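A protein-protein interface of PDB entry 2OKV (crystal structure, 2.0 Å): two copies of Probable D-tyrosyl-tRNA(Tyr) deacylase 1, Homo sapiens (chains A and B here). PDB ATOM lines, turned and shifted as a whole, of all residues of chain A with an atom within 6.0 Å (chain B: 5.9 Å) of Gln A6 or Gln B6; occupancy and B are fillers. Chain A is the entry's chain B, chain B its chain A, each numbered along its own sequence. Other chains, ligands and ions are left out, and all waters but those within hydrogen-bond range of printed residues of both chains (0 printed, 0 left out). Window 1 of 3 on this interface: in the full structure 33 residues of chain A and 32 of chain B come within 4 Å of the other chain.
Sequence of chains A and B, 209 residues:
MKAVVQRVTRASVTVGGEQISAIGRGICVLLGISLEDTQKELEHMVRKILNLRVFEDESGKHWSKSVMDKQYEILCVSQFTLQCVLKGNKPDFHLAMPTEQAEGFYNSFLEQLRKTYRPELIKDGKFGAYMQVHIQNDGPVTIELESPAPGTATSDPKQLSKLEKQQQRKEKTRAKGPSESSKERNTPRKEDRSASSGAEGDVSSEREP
Gln A6 touches Ile B135 (OE1 to CD1, 3.6 Å).
Gln B6 touches Leu A30 (NE2 to CD1, 3.98 Å).
OG1 of Thr B142 touches CD1 of Leu A30, at 3.2 Å.
Gln B6 touches Ile A135 (NE2 to CD1, 3.7 Å).
Leu B30 touches Thr A142.
Of the 15 printed residues of chain A, 4 touch a printed residue of chain B.
Hydrophobic or aromatic side chains of chain A that line the printed part of chain B: Leu A30 and Ile A135.
Along chain A the printed residues that touch a printed residue of chain B span positions 6 to 142.
Along chain B the printed residues that touch a printed residue of chain A span positions 6 to 142.
Among the printed residues, 7 pairs touch across the chains.
Among the printed residues, no Asp or Glu carboxylate lies within 4 Å of a Lys or Arg side-chain nitrogen of the other chain.
O of Ile A135 lies within hydrogen-bond range of N of Ile B135, 2.7 Å away.
The side-chain amide nitrogen (NE2) of Gln A6 lies close to the side-chain amide nitrogen (NE2) of Gln B6 (3.0 Å).
The side-chain amide nitrogen of Asn B137 lies within hydrogen-bond range of the side-chain hydroxyl of Thr B142.
The backbone carbonyl oxygen of Gln B6 sits at hydrogen-bond distance from the backbone NH of Cys B28.
The backbone carbonyl oxygen (O) of Val B4 sits at hydrogen-bond distance from the backbone NH (N) of Leu B30 (2.9 Å).
ND2 of Asn A137 lies within hydrogen-bond range of OG1 of Thr A142, at 3.1 Å.
ND2 of Asn B137 lies close to NE2 of Gln B6 (2.9 Å).
The side-chain amide oxygen of Gln A6 sits at hydrogen-bond distance from the side-chain amide nitrogen of Asn A137 (2.9 Å).
Of the printed residues of chain B, Thr A142 touches Leu B30 (3.4 Å).
Of the printed residues of chain B, Ile A135 touches Gln B6 (3.7 Å) and Ile B135 (2.7 Å).
Arg A7 touches none of the printed residues of chain B.
The nearest printed residue of chain A that does not touch Thr B142 is Val A4 (4.4 Å).
Gln B6 touches its own counterpart, Gln A6.
Gln A6 touches Ile B135, and with the chains exchanged Ile A135 touches Gln B6.
Leu A30 touches Gln B6, but with the chains exchanged Gln A6 does not touch Leu B30 (4.2 Å).
Leu A30 touches Thr B142, and with the chains exchanged Thr A142 touches Leu B30.
Positions printed for both chains: 4, 5, 6, 7, 8, 26, 27, 28, 29, 30, 135, 137, 141, 142 and 143.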
ATOM      1  N   VAL A   4      -5.194   6.114 -17.984  1.00  0.00           N
ATOM      2  CA  VAL A   4      -5.950   6.502 -19.173  1.00  0.00           C
ATOM      3  C   VAL A   4      -7.186   5.632 -19.191  1.00  0.00           C
ATOM      4  O   VAL A   4      -7.100   4.411 -19.154  1.00  0.00           O
ATOM      5  CB  VAL A   4      -5.142   6.394 -20.482  1.00  0.00           C
ATOM      6  CG1 VAL A   4      -6.075   6.579 -21.718  1.00  0.00           C
ATOM      7  CG2 VAL A   4      -4.019   7.440 -20.493  1.00  0.00           C
ATOM      8  N   VAL A   5      -8.340   6.286 -19.227  1.00  0.00           N
ATOM      9  CA  VAL A   5      -9.623   5.619 -19.148  1.00  0.00           C
ATOM     10  C   VAL A   5     -10.336   5.797 -20.482  1.00  0.00           C
ATOM     11  O   VAL A   5     -10.508   6.927 -20.978  1.00  0.00           O
ATOM     12  CB  VAL A   5     -10.477   6.214 -18.000  1.00  0.00           C
ATOM     13  CG1 VAL A   5     -11.848   5.594 -17.984  1.00  0.00           C
ATOM     14  CG2 VAL A   5      -9.788   6.006 -16.637  1.00  0.00           C
ATOM     15  N   GLN A   6     -10.719   4.685 -21.093  1.00  0.00           N
ATOM     16  CA  GLN A   6     -11.438   4.750 -22.367  1.00  0.00           C
ATOM     17  C   GLN A   6     -12.807   4.109 -22.210  1.00  0.00           C
ATOM     18  O   GLN A   6     -12.910   2.996 -21.706  1.00  0.00           O
ATOM     19  CB  GLN A   6     -10.646   4.044 -23.476  1.00  0.00           C
ATOM     20  CG  GLN A   6      -9.336   4.764 -23.834  1.00  0.00           C
ATOM     21  CD  GLN A   6      -8.513   4.028 -24.881  1.00  0.00           C
ATOM     22  OE1 GLN A   6      -8.794   4.107 -26.084  1.00  0.00           O
ATOM     23  NE2 GLN A   6      -7.440   3.348 -24.427  1.00  0.00           N
ATOM     24  N   ARG A   7     -13.850   4.806 -22.646  1.00  0.00           N
ATOM     25  CA  ARG A   7     -15.198   4.250 -22.593  1.00  0.00           C
ATOM     26  C   ARG A   7     -15.315   3.250 -23.727  1.00  0.00           C
ATOM     27  O   ARG A   7     -14.987   3.569 -24.862  1.00  0.00           O
ATOM     28  CB  ARG A   7     -16.257   5.347 -22.753  1.00  0.00           C
ATOM     29  CG  ARG A   7     -17.696   4.822 -22.740  1.00  0.00           C
ATOM     30  CD  ARG A   7     -18.731   5.931 -22.820  1.00  0.00           C
ATOM     31  NE  ARG A   7     -18.825   6.490 -24.169  1.00  0.00           N
ATOM     32  CZ  ARG A   7     -19.655   7.461 -24.527  1.00  0.00           C
ATOM     33  NH1 ARG A   7     -20.459   8.024 -23.627  1.00  0.00           N
ATOM     34  NH2 ARG A   7     -19.665   7.888 -25.790  1.00  0.00           N
ATOM     35  N   VAL A   8     -15.800   2.049 -23.431  1.00  0.00           N
ATOM     36  CA  VAL A   8     -15.842   0.996 -24.457  1.00  0.00           C
ATOM     37  C   VAL A   8     -17.242   0.413 -24.698  1.00  0.00           C
ATOM     38  O   VAL A   8     -18.070   0.352 -23.757  1.00  0.00           O
ATOM     39  CB  VAL A   8     -14.830  -0.144 -24.149  1.00  0.00           C
ATOM     40  CG1 VAL A   8     -13.397   0.394 -24.123  1.00  0.00           C
ATOM     41  CG2 VAL A   8     -15.170  -0.866 -22.840  1.00  0.00           C
ATOM     42  N   GLY A  26     -18.632  -0.688 -20.808  1.00  0.00           N
ATOM     43  CA  GLY A  26     -17.976  -0.245 -19.596  1.00  0.00           C
ATOM     44  C   GLY A  26     -16.743   0.591 -19.894  1.00  0.00           C
ATOM     45  O   GLY A  26     -16.751   1.460 -20.769  1.00  0.00           O
ATOM     46  N   ILE A  27     -15.665   0.296 -19.187  1.00  0.00           N
ATOM     47  CA  ILE A  27     -14.487   1.151 -19.208  1.00  0.00           C
ATOM     48  C   ILE A  27     -13.189   0.313 -19.208  1.00  0.00           C
ATOM     49  O   ILE A  27     -13.098  -0.679 -18.496  1.00  0.00           O
ATOM     50  CB  ILE A  27     -14.668   2.168 -18.036  1.00  0.00           C
ATOM     51  CG1 ILE A  27     -14.464   3.607 -18.462  1.00  0.00           C
ATOM     52  CG2 ILE A  27     -14.116   1.749 -16.654  1.00  0.00           C
ATOM     53  CD1 ILE A  27     -15.197   4.520 -17.583  1.00  0.00           C
ATOM     54  N   CYS A  28     -12.227   0.691 -20.054  1.00  0.00           N
ATOM     55  CA  CYS A  28     -10.891   0.088 -20.055  1.00  0.00           C
ATOM     56  C   CYS A  28      -9.934   1.088 -19.434  1.00  0.00           C
ATOM     57  O   CYS A  28      -9.831   2.225 -19.885  1.00  0.00           O
ATOM     58  CB  CYS A  28     -10.424  -0.275 -21.485  1.00  0.00           C
ATOM     59  SG  CYS A  28      -8.758  -1.026 -21.563  1.00  0.00           S
ATOM     60  N   VAL A  29      -9.241   0.654 -18.396  1.00  0.00           N
ATOM     61  CA  VAL A  29      -8.329   1.508 -17.658  1.00  0.00           C
ATOM     62  C   VAL A  29      -6.911   0.999 -17.884  1.00  0.00           C
ATOM     63  O   VAL A  29      -6.601  -0.171 -17.607  1.00  0.00           O
ATOM     64  CB  VAL A  29      -8.651   1.495 -16.139  1.00  0.00           C
ATOM     65  CG1 VAL A  29      -7.682   2.405 -15.363  1.00  0.00           C
ATOM     66  CG2 VAL A  29     -10.113   1.898 -15.899  1.00  0.00           C
ATOM     67  N   LEU A  30      -6.061   1.876 -18.411  1.00  0.00           N
ATOM     68  CA  LEU A  30      -4.643   1.604 -18.481  1.00  0.00           C
ATOM     69  C   LEU A  30      -3.995   2.306 -17.310  1.00  0.00           C
ATOM     70  O   LEU A  30      -4.070   3.535 -17.203  1.00  0.00           O
ATOM     71  CB  LEU A  30      -4.071   2.086 -19.815  1.00  0.00           C
ATOM     72  CG  LEU A  30      -4.647   1.340 -21.028  1.00  0.00           C
ATOM     73  CD1 LEU A  30      -4.387   2.105 -22.308  1.00  0.00           C
ATOM     74  CD2 LEU A  30      -4.063  -0.099 -21.139  1.00  0.00           C
ATOM     75  N   ILE A 135      -9.554  -2.701 -27.830  1.00  0.00           N
ATOM     76  CA  ILE A 135     -10.332  -1.659 -27.193  1.00  0.00           C
ATOM     77  C   ILE A 135     -11.288  -1.075 -28.218  1.00  0.00           C
ATOM     78  O   ILE A 135     -10.845  -0.423 -29.171  1.00  0.00           O
ATOM     79  CB  ILE A 135      -9.416  -0.540 -26.613  1.00  0.00           C
ATOM     80  CG1 ILE A 135      -8.434  -1.147 -25.597  1.00  0.00           C
ATOM     81  CG2 ILE A 135     -10.260   0.566 -25.959  1.00  0.00           C
ATOM     82  CD1 ILE A 135      -7.392  -0.193 -25.050  1.00  0.00           C
ATOM     83  N   ASN A 137     -13.296   1.714 -28.481  1.00  0.00           N
ATOM     84  CA  ASN A 137     -13.521   2.983 -27.814  1.00  0.00           C
ATOM     85  C   ASN A 137     -14.809   3.620 -28.354  1.00  0.00           C
ATOM     86  O   ASN A 137     -14.898   3.935 -29.537  1.00  0.00           O
ATOM     87  CB  ASN A 137     -12.305   3.897 -28.006  1.00  0.00           C
ATOM     88  CG  ASN A 137     -12.347   5.146 -27.110  1.00  0.00           C
ATOM     89  OD1 ASN A 137     -13.400   5.706 -26.857  1.00  0.00           O
ATOM     90  ND2 ASN A 137     -11.186   5.566 -26.622  1.00  0.00           N
ATOM     91  N   VAL A 141     -14.377   8.264 -26.291  1.00  0.00           N
ATOM     92  CA  VAL A 141     -14.318   9.043 -25.037  1.00  0.00           C
ATOM     93  C   VAL A 141     -13.079   8.564 -24.287  1.00  0.00           C
ATOM     94  O   VAL A 141     -12.931   7.358 -24.004  1.00  0.00           O
ATOM     95  CB  VAL A 141     -15.582   8.872 -24.158  1.00  0.00           C
ATOM     96  CG1 VAL A 141     -15.366   9.495 -22.778  1.00  0.00           C
ATOM     97  CG2 VAL A 141     -16.771   9.533 -24.811  1.00  0.00           C
ATOM     98  N   THR A 142     -12.187   9.500 -23.977  1.00  0.00           N
ATOM     99  CA  THR A 142     -10.907   9.135 -23.347  1.00  0.00           C
ATOM    100  C   THR A 142     -10.568  10.166 -22.282  1.00  0.00           C
ATOM    101  O   THR A 142     -10.533  11.346 -22.564  1.00  0.00           O
ATOM    102  CB  THR A 142      -9.771   9.114 -24.400  1.00  0.00           C
ATOM    103  OG1 THR A 142     -10.166   8.327 -25.531  1.00  0.00           O
ATOM    104  CG2 THR A 142      -8.463   8.548 -23.806  1.00  0.00           C
ATOM    105  N   ILE A 143     -10.291   9.715 -21.062  1.00  0.00           N
ATOM    106  CA  ILE A 143     -10.058  10.640 -19.957  1.00  0.00           C
ATOM    107  C   ILE A 143      -8.733  10.301 -19.280  1.00  0.00           C
ATOM    108  O   ILE A 143      -8.477   9.132 -18.994  1.00  0.00           O
ATOM    109  CB  ILE A 143     -11.209  10.547 -18.907  1.00  0.00           C
ATOM    110  CG1 ILE A 143     -12.555  11.006 -19.522  1.00  0.00           C
ATOM    111  CG2 ILE A 143     -10.859  11.329 -17.604  1.00  0.00           C
ATOM    112  CD1 ILE A 143     -12.670  12.494 -19.798  1.00  0.00           C
ATOM    113  N   VAL B   4      -3.072  11.300 -26.613  1.00  0.00           N
ATOM    114  CA  VAL B   4      -2.807   9.937 -26.114  1.00  0.00           C
ATOM    115  C   VAL B   4      -2.415   9.089 -27.313  1.00  0.00           C
ATOM    116  O   VAL B   4      -3.164   8.982 -28.291  1.00  0.00           O
ATOM    117  CB  VAL B   4      -4.004   9.301 -25.386  1.00  0.00           C
ATOM    118  CG1 VAL B   4      -3.745   7.801 -25.095  1.00  0.00           C
ATOM    119  CG2 VAL B   4      -4.300  10.044 -24.094  1.00  0.00           C
ATOM    120  N   VAL B   5      -1.231   8.499 -27.232  1.00  0.00           N
ATOM    121  CA  VAL B   5      -0.712   7.728 -28.344  1.00  0.00           C
ATOM    122  C   VAL B   5      -0.722   6.270 -27.917  1.00  0.00           C
ATOM    123  O   VAL B   5      -0.167   5.930 -26.870  1.00  0.00           O
ATOM    124  CB  VAL B   5       0.732   8.168 -28.709  1.00  0.00           C
ATOM    125  CG1 VAL B   5       1.276   7.352 -29.907  1.00  0.00           C
ATOM    126  CG2 VAL B   5       0.767   9.672 -29.040  1.00  0.00           C
ATOM    127  N   GLN B   6      -1.370   5.422 -28.717  1.00  0.00           N
ATOM    128  CA  GLN B   6      -1.361   3.972 -28.475  1.00  0.00           C
ATOM    129  C   GLN B   6      -0.690   3.245 -29.623  1.00  0.00           C
ATOM    130  O   GLN B   6      -1.057   3.451 -30.782  1.00  0.00           O
ATOM    131  CB  GLN B   6      -2.788   3.478 -28.277  1.00  0.00           C
ATOM    132  CG  GLN B   6      -3.390   4.013 -26.964  1.00  0.00           C
ATOM    133  CD  GLN B   6      -4.857   3.704 -26.806  1.00  0.00           C
ATOM    134  OE1 GLN B   6      -5.744   4.516 -27.196  1.00  0.00           O
ATOM    135  NE2 GLN B   6      -5.144   2.565 -26.191  1.00  0.00           N
ATOM    136  N   ARG B   7       0.316   2.428 -29.303  1.00  0.00           N
ATOM    137  CA  ARG B   7       0.942   1.557 -30.308  1.00  0.00           C
ATOM    138  C   ARG B   7      -0.075   0.490 -30.681  1.00  0.00           C
ATOM    139  O   ARG B   7      -0.689  -0.096 -29.783  1.00  0.00           O
ATOM    140  CB  ARG B   7       2.187   0.884 -29.730  1.00  0.00           C
ATOM    141  CG  ARG B   7       2.972   0.077 -30.799  1.00  0.00           C
ATOM    142  CD  ARG B   7       4.313  -0.330 -30.252  1.00  0.00           C
ATOM    143  NE  ARG B   7       4.164  -1.474 -29.367  1.00  0.00           N
ATOM    144  CZ  ARG B   7       5.169  -2.194 -28.885  1.00  0.00           C
ATOM    145  NH1 ARG B   7       6.439  -1.883 -29.168  1.00  0.00           N
ATOM    146  NH2 ARG B   7       4.892  -3.234 -28.109  1.00  0.00           N
ATOM    147  N   VAL B   8      -0.267   0.233 -31.981  1.00  0.00           N
ATOM    148  CA  VAL B   8      -1.306  -0.701 -32.413  1.00  0.00           C
ATOM    149  C   VAL B   8      -0.779  -1.770 -33.362  1.00  0.00           C
ATOM    150  O   VAL B   8       0.159  -1.517 -34.132  1.00  0.00           O
ATOM    151  CB  VAL B   8      -2.541   0.023 -33.057  1.00  0.00           C
ATOM    152  CG1 VAL B   8      -3.178   1.023 -32.064  1.00  0.00           C
ATOM    153  CG2 VAL B   8      -2.167   0.733 -34.369  1.00  0.00           C
ATOM    154  N   GLY B  26       1.266   0.423 -36.358  1.00  0.00           N
ATOM    155  CA  GLY B  26       1.608   1.832 -36.216  1.00  0.00           C
ATOM    156  C   GLY B  26       1.094   2.386 -34.899  1.00  0.00           C
ATOM    157  O   GLY B  26       1.204   1.740 -33.855  1.00  0.00           O
ATOM    158  N   ILE B  27       0.565   3.606 -34.938  1.00  0.00           N
ATOM    159  CA  ILE B  27       0.049   4.256 -33.726  1.00  0.00           C
ATOM    160  C   ILE B  27      -1.331   4.830 -33.983  1.00  0.00           C
ATOM    161  O   ILE B  27      -1.618   5.259 -35.097  1.00  0.00           O
ATOM    162  CB  ILE B  27       0.953   5.412 -33.240  1.00  0.00           C
ATOM    163  CG1 ILE B  27       1.338   6.342 -34.414  1.00  0.00           C
ATOM    164  CG2 ILE B  27       2.190   4.853 -32.549  1.00  0.00           C
ATOM    165  CD1 ILE B  27       2.154   7.582 -34.025  1.00  0.00           C
ATOM    166  N   CYS B  28      -2.185   4.795 -32.956  1.00  0.00           N
ATOM    167  CA  CYS B  28      -3.451   5.512 -32.982  1.00  0.00           C
ATOM    168  C   CYS B  28      -3.286   6.708 -32.056  1.00  0.00           C
ATOM    169  O   CYS B  28      -2.943   6.539 -30.872  1.00  0.00           O
ATOM    170  CB  CYS B  28      -4.584   4.609 -32.489  1.00  0.00           C
ATOM    171  SG  CYS B  28      -6.194   5.481 -32.349  1.00  0.00           S
ATOM    172  N   VAL B  29      -3.507   7.905 -32.599  1.00  0.00           N
ATOM    173  CA  VAL B  29      -3.299   9.154 -31.884  1.00  0.00           C
ATOM    174  C   VAL B  29      -4.672   9.785 -31.597  1.00  0.00           C
ATOM    175  O   VAL B  29      -5.444  10.074 -32.527  1.00  0.00           O
ATOM    176  CB  VAL B  29      -2.471  10.164 -32.712  1.00  0.00           C
ATOM    177  CG1 VAL B  29      -2.310  11.469 -31.971  1.00  0.00           C
ATOM    178  CG2 VAL B  29      -1.090   9.584 -33.069  1.00  0.00           C
ATOM    179  N   LEU B  30      -4.979   9.979 -30.319  1.00  0.00           N
ATOM    180  CA  LEU B  30      -6.204  10.704 -29.932  1.00  0.00           C
ATOM    181  C   LEU B  30      -5.789  12.115 -29.560  1.00  0.00           C
ATOM    182  O   LEU B  30      -5.000  12.301 -28.642  1.00  0.00           O
ATOM    183  CB  LEU B  30      -6.903  10.005 -28.748  1.00  0.00           C
ATOM    184  CG  LEU B  30      -7.511   8.627 -29.067  1.00  0.00           C
ATOM    185  CD1 LEU B  30      -7.739   7.748 -27.837  1.00  0.00           C
ATOM    186  CD2 LEU B  30      -8.821   8.797 -29.857  1.00  0.00           C
ATOM    187  N   ILE B 135      -9.242  -0.243 -31.369  1.00  0.00           N
ATOM    188  CA  ILE B 135      -7.804  -0.055 -31.145  1.00  0.00           C
ATOM    189  C   ILE B 135      -7.214  -1.358 -30.619  1.00  0.00           C
ATOM    190  O   ILE B 135      -7.576  -1.801 -29.529  1.00  0.00           O
ATOM    191  CB  ILE B 135      -7.541   1.113 -30.120  1.00  0.00           C
ATOM    192  CG1 ILE B 135      -8.111   2.443 -30.651  1.00  0.00           C
ATOM    193  CG2 ILE B 135      -6.057   1.233 -29.815  1.00  0.00           C
ATOM    194  CD1 ILE B 135      -8.183   3.611 -29.622  1.00  0.00           C
ATOM    195  N   ASN B 137      -4.371  -2.389 -29.083  1.00  0.00           N
ATOM    196  CA  ASN B 137      -3.202  -1.844 -28.435  1.00  0.00           C
ATOM    197  C   ASN B 137      -2.178  -2.962 -28.250  1.00  0.00           C
ATOM    198  O   ASN B 137      -2.453  -3.980 -27.593  1.00  0.00           O
ATOM    199  CB  ASN B 137      -3.583  -1.147 -27.124  1.00  0.00           C
ATOM    200  CG  ASN B 137      -2.460  -0.298 -26.575  1.00  0.00           C
ATOM    201  OD1 ASN B 137      -1.294  -0.660 -26.682  1.00  0.00           O
ATOM    202  ND2 ASN B 137      -2.805   0.834 -25.965  1.00  0.00           N
ATOM    203  N   VAL B 141       1.078  -0.504 -25.247  1.00  0.00           N
ATOM    204  CA  VAL B 141       1.999   0.626 -25.087  1.00  0.00           C
ATOM    205  C   VAL B 141       1.187   1.896 -25.264  1.00  0.00           C
ATOM    206  O   VAL B 141       0.558   2.089 -26.314  1.00  0.00           O
ATOM    207  CB  VAL B 141       3.176   0.572 -26.086  1.00  0.00           C
ATOM    208  CG1 VAL B 141       3.948   1.903 -26.101  1.00  0.00           C
ATOM    209  CG2 VAL B 141       4.139  -0.575 -25.724  1.00  0.00           C
ATOM    210  N   THR B 142       1.197   2.750 -24.238  1.00  0.00           N
ATOM    211  CA  THR B 142       0.407   3.989 -24.236  1.00  0.00           C
ATOM    212  C   THR B 142       1.240   5.139 -23.660  1.00  0.00           C
ATOM    213  O   THR B 142       1.827   5.025 -22.580  1.00  0.00           O
ATOM    214  CB  THR B 142      -0.868   3.813 -23.379  1.00  0.00           C
ATOM    215  OG1 THR B 142      -1.529   2.593 -23.745  1.00  0.00           O
ATOM    216  CG2 THR B 142      -1.852   5.004 -23.505  1.00  0.00           C
ATOM    217  N   ILE B 143       1.257   6.256 -24.374  1.00  0.00           N
ATOM    218  CA  ILE B 143       2.069   7.410 -24.011  1.00  0.00           C
ATOM    219  C   ILE B 143       1.182   8.655 -24.048  1.00  0.00           C
ATOM    220  O   ILE B 143       0.459   8.865 -25.021  1.00  0.00           O
ATOM    221  CB  ILE B 143       3.233   7.595 -25.045  1.00  0.00           C
ATOM    222  CG1 ILE B 143       4.159   6.369 -25.083  1.00  0.00           C
ATOM    223  CG2 ILE B 143       4.045   8.896 -24.796  1.00  0.00           C
ATOM    224  CD1 ILE B 143       5.062   6.180 -23.832  1.00  0.00           C
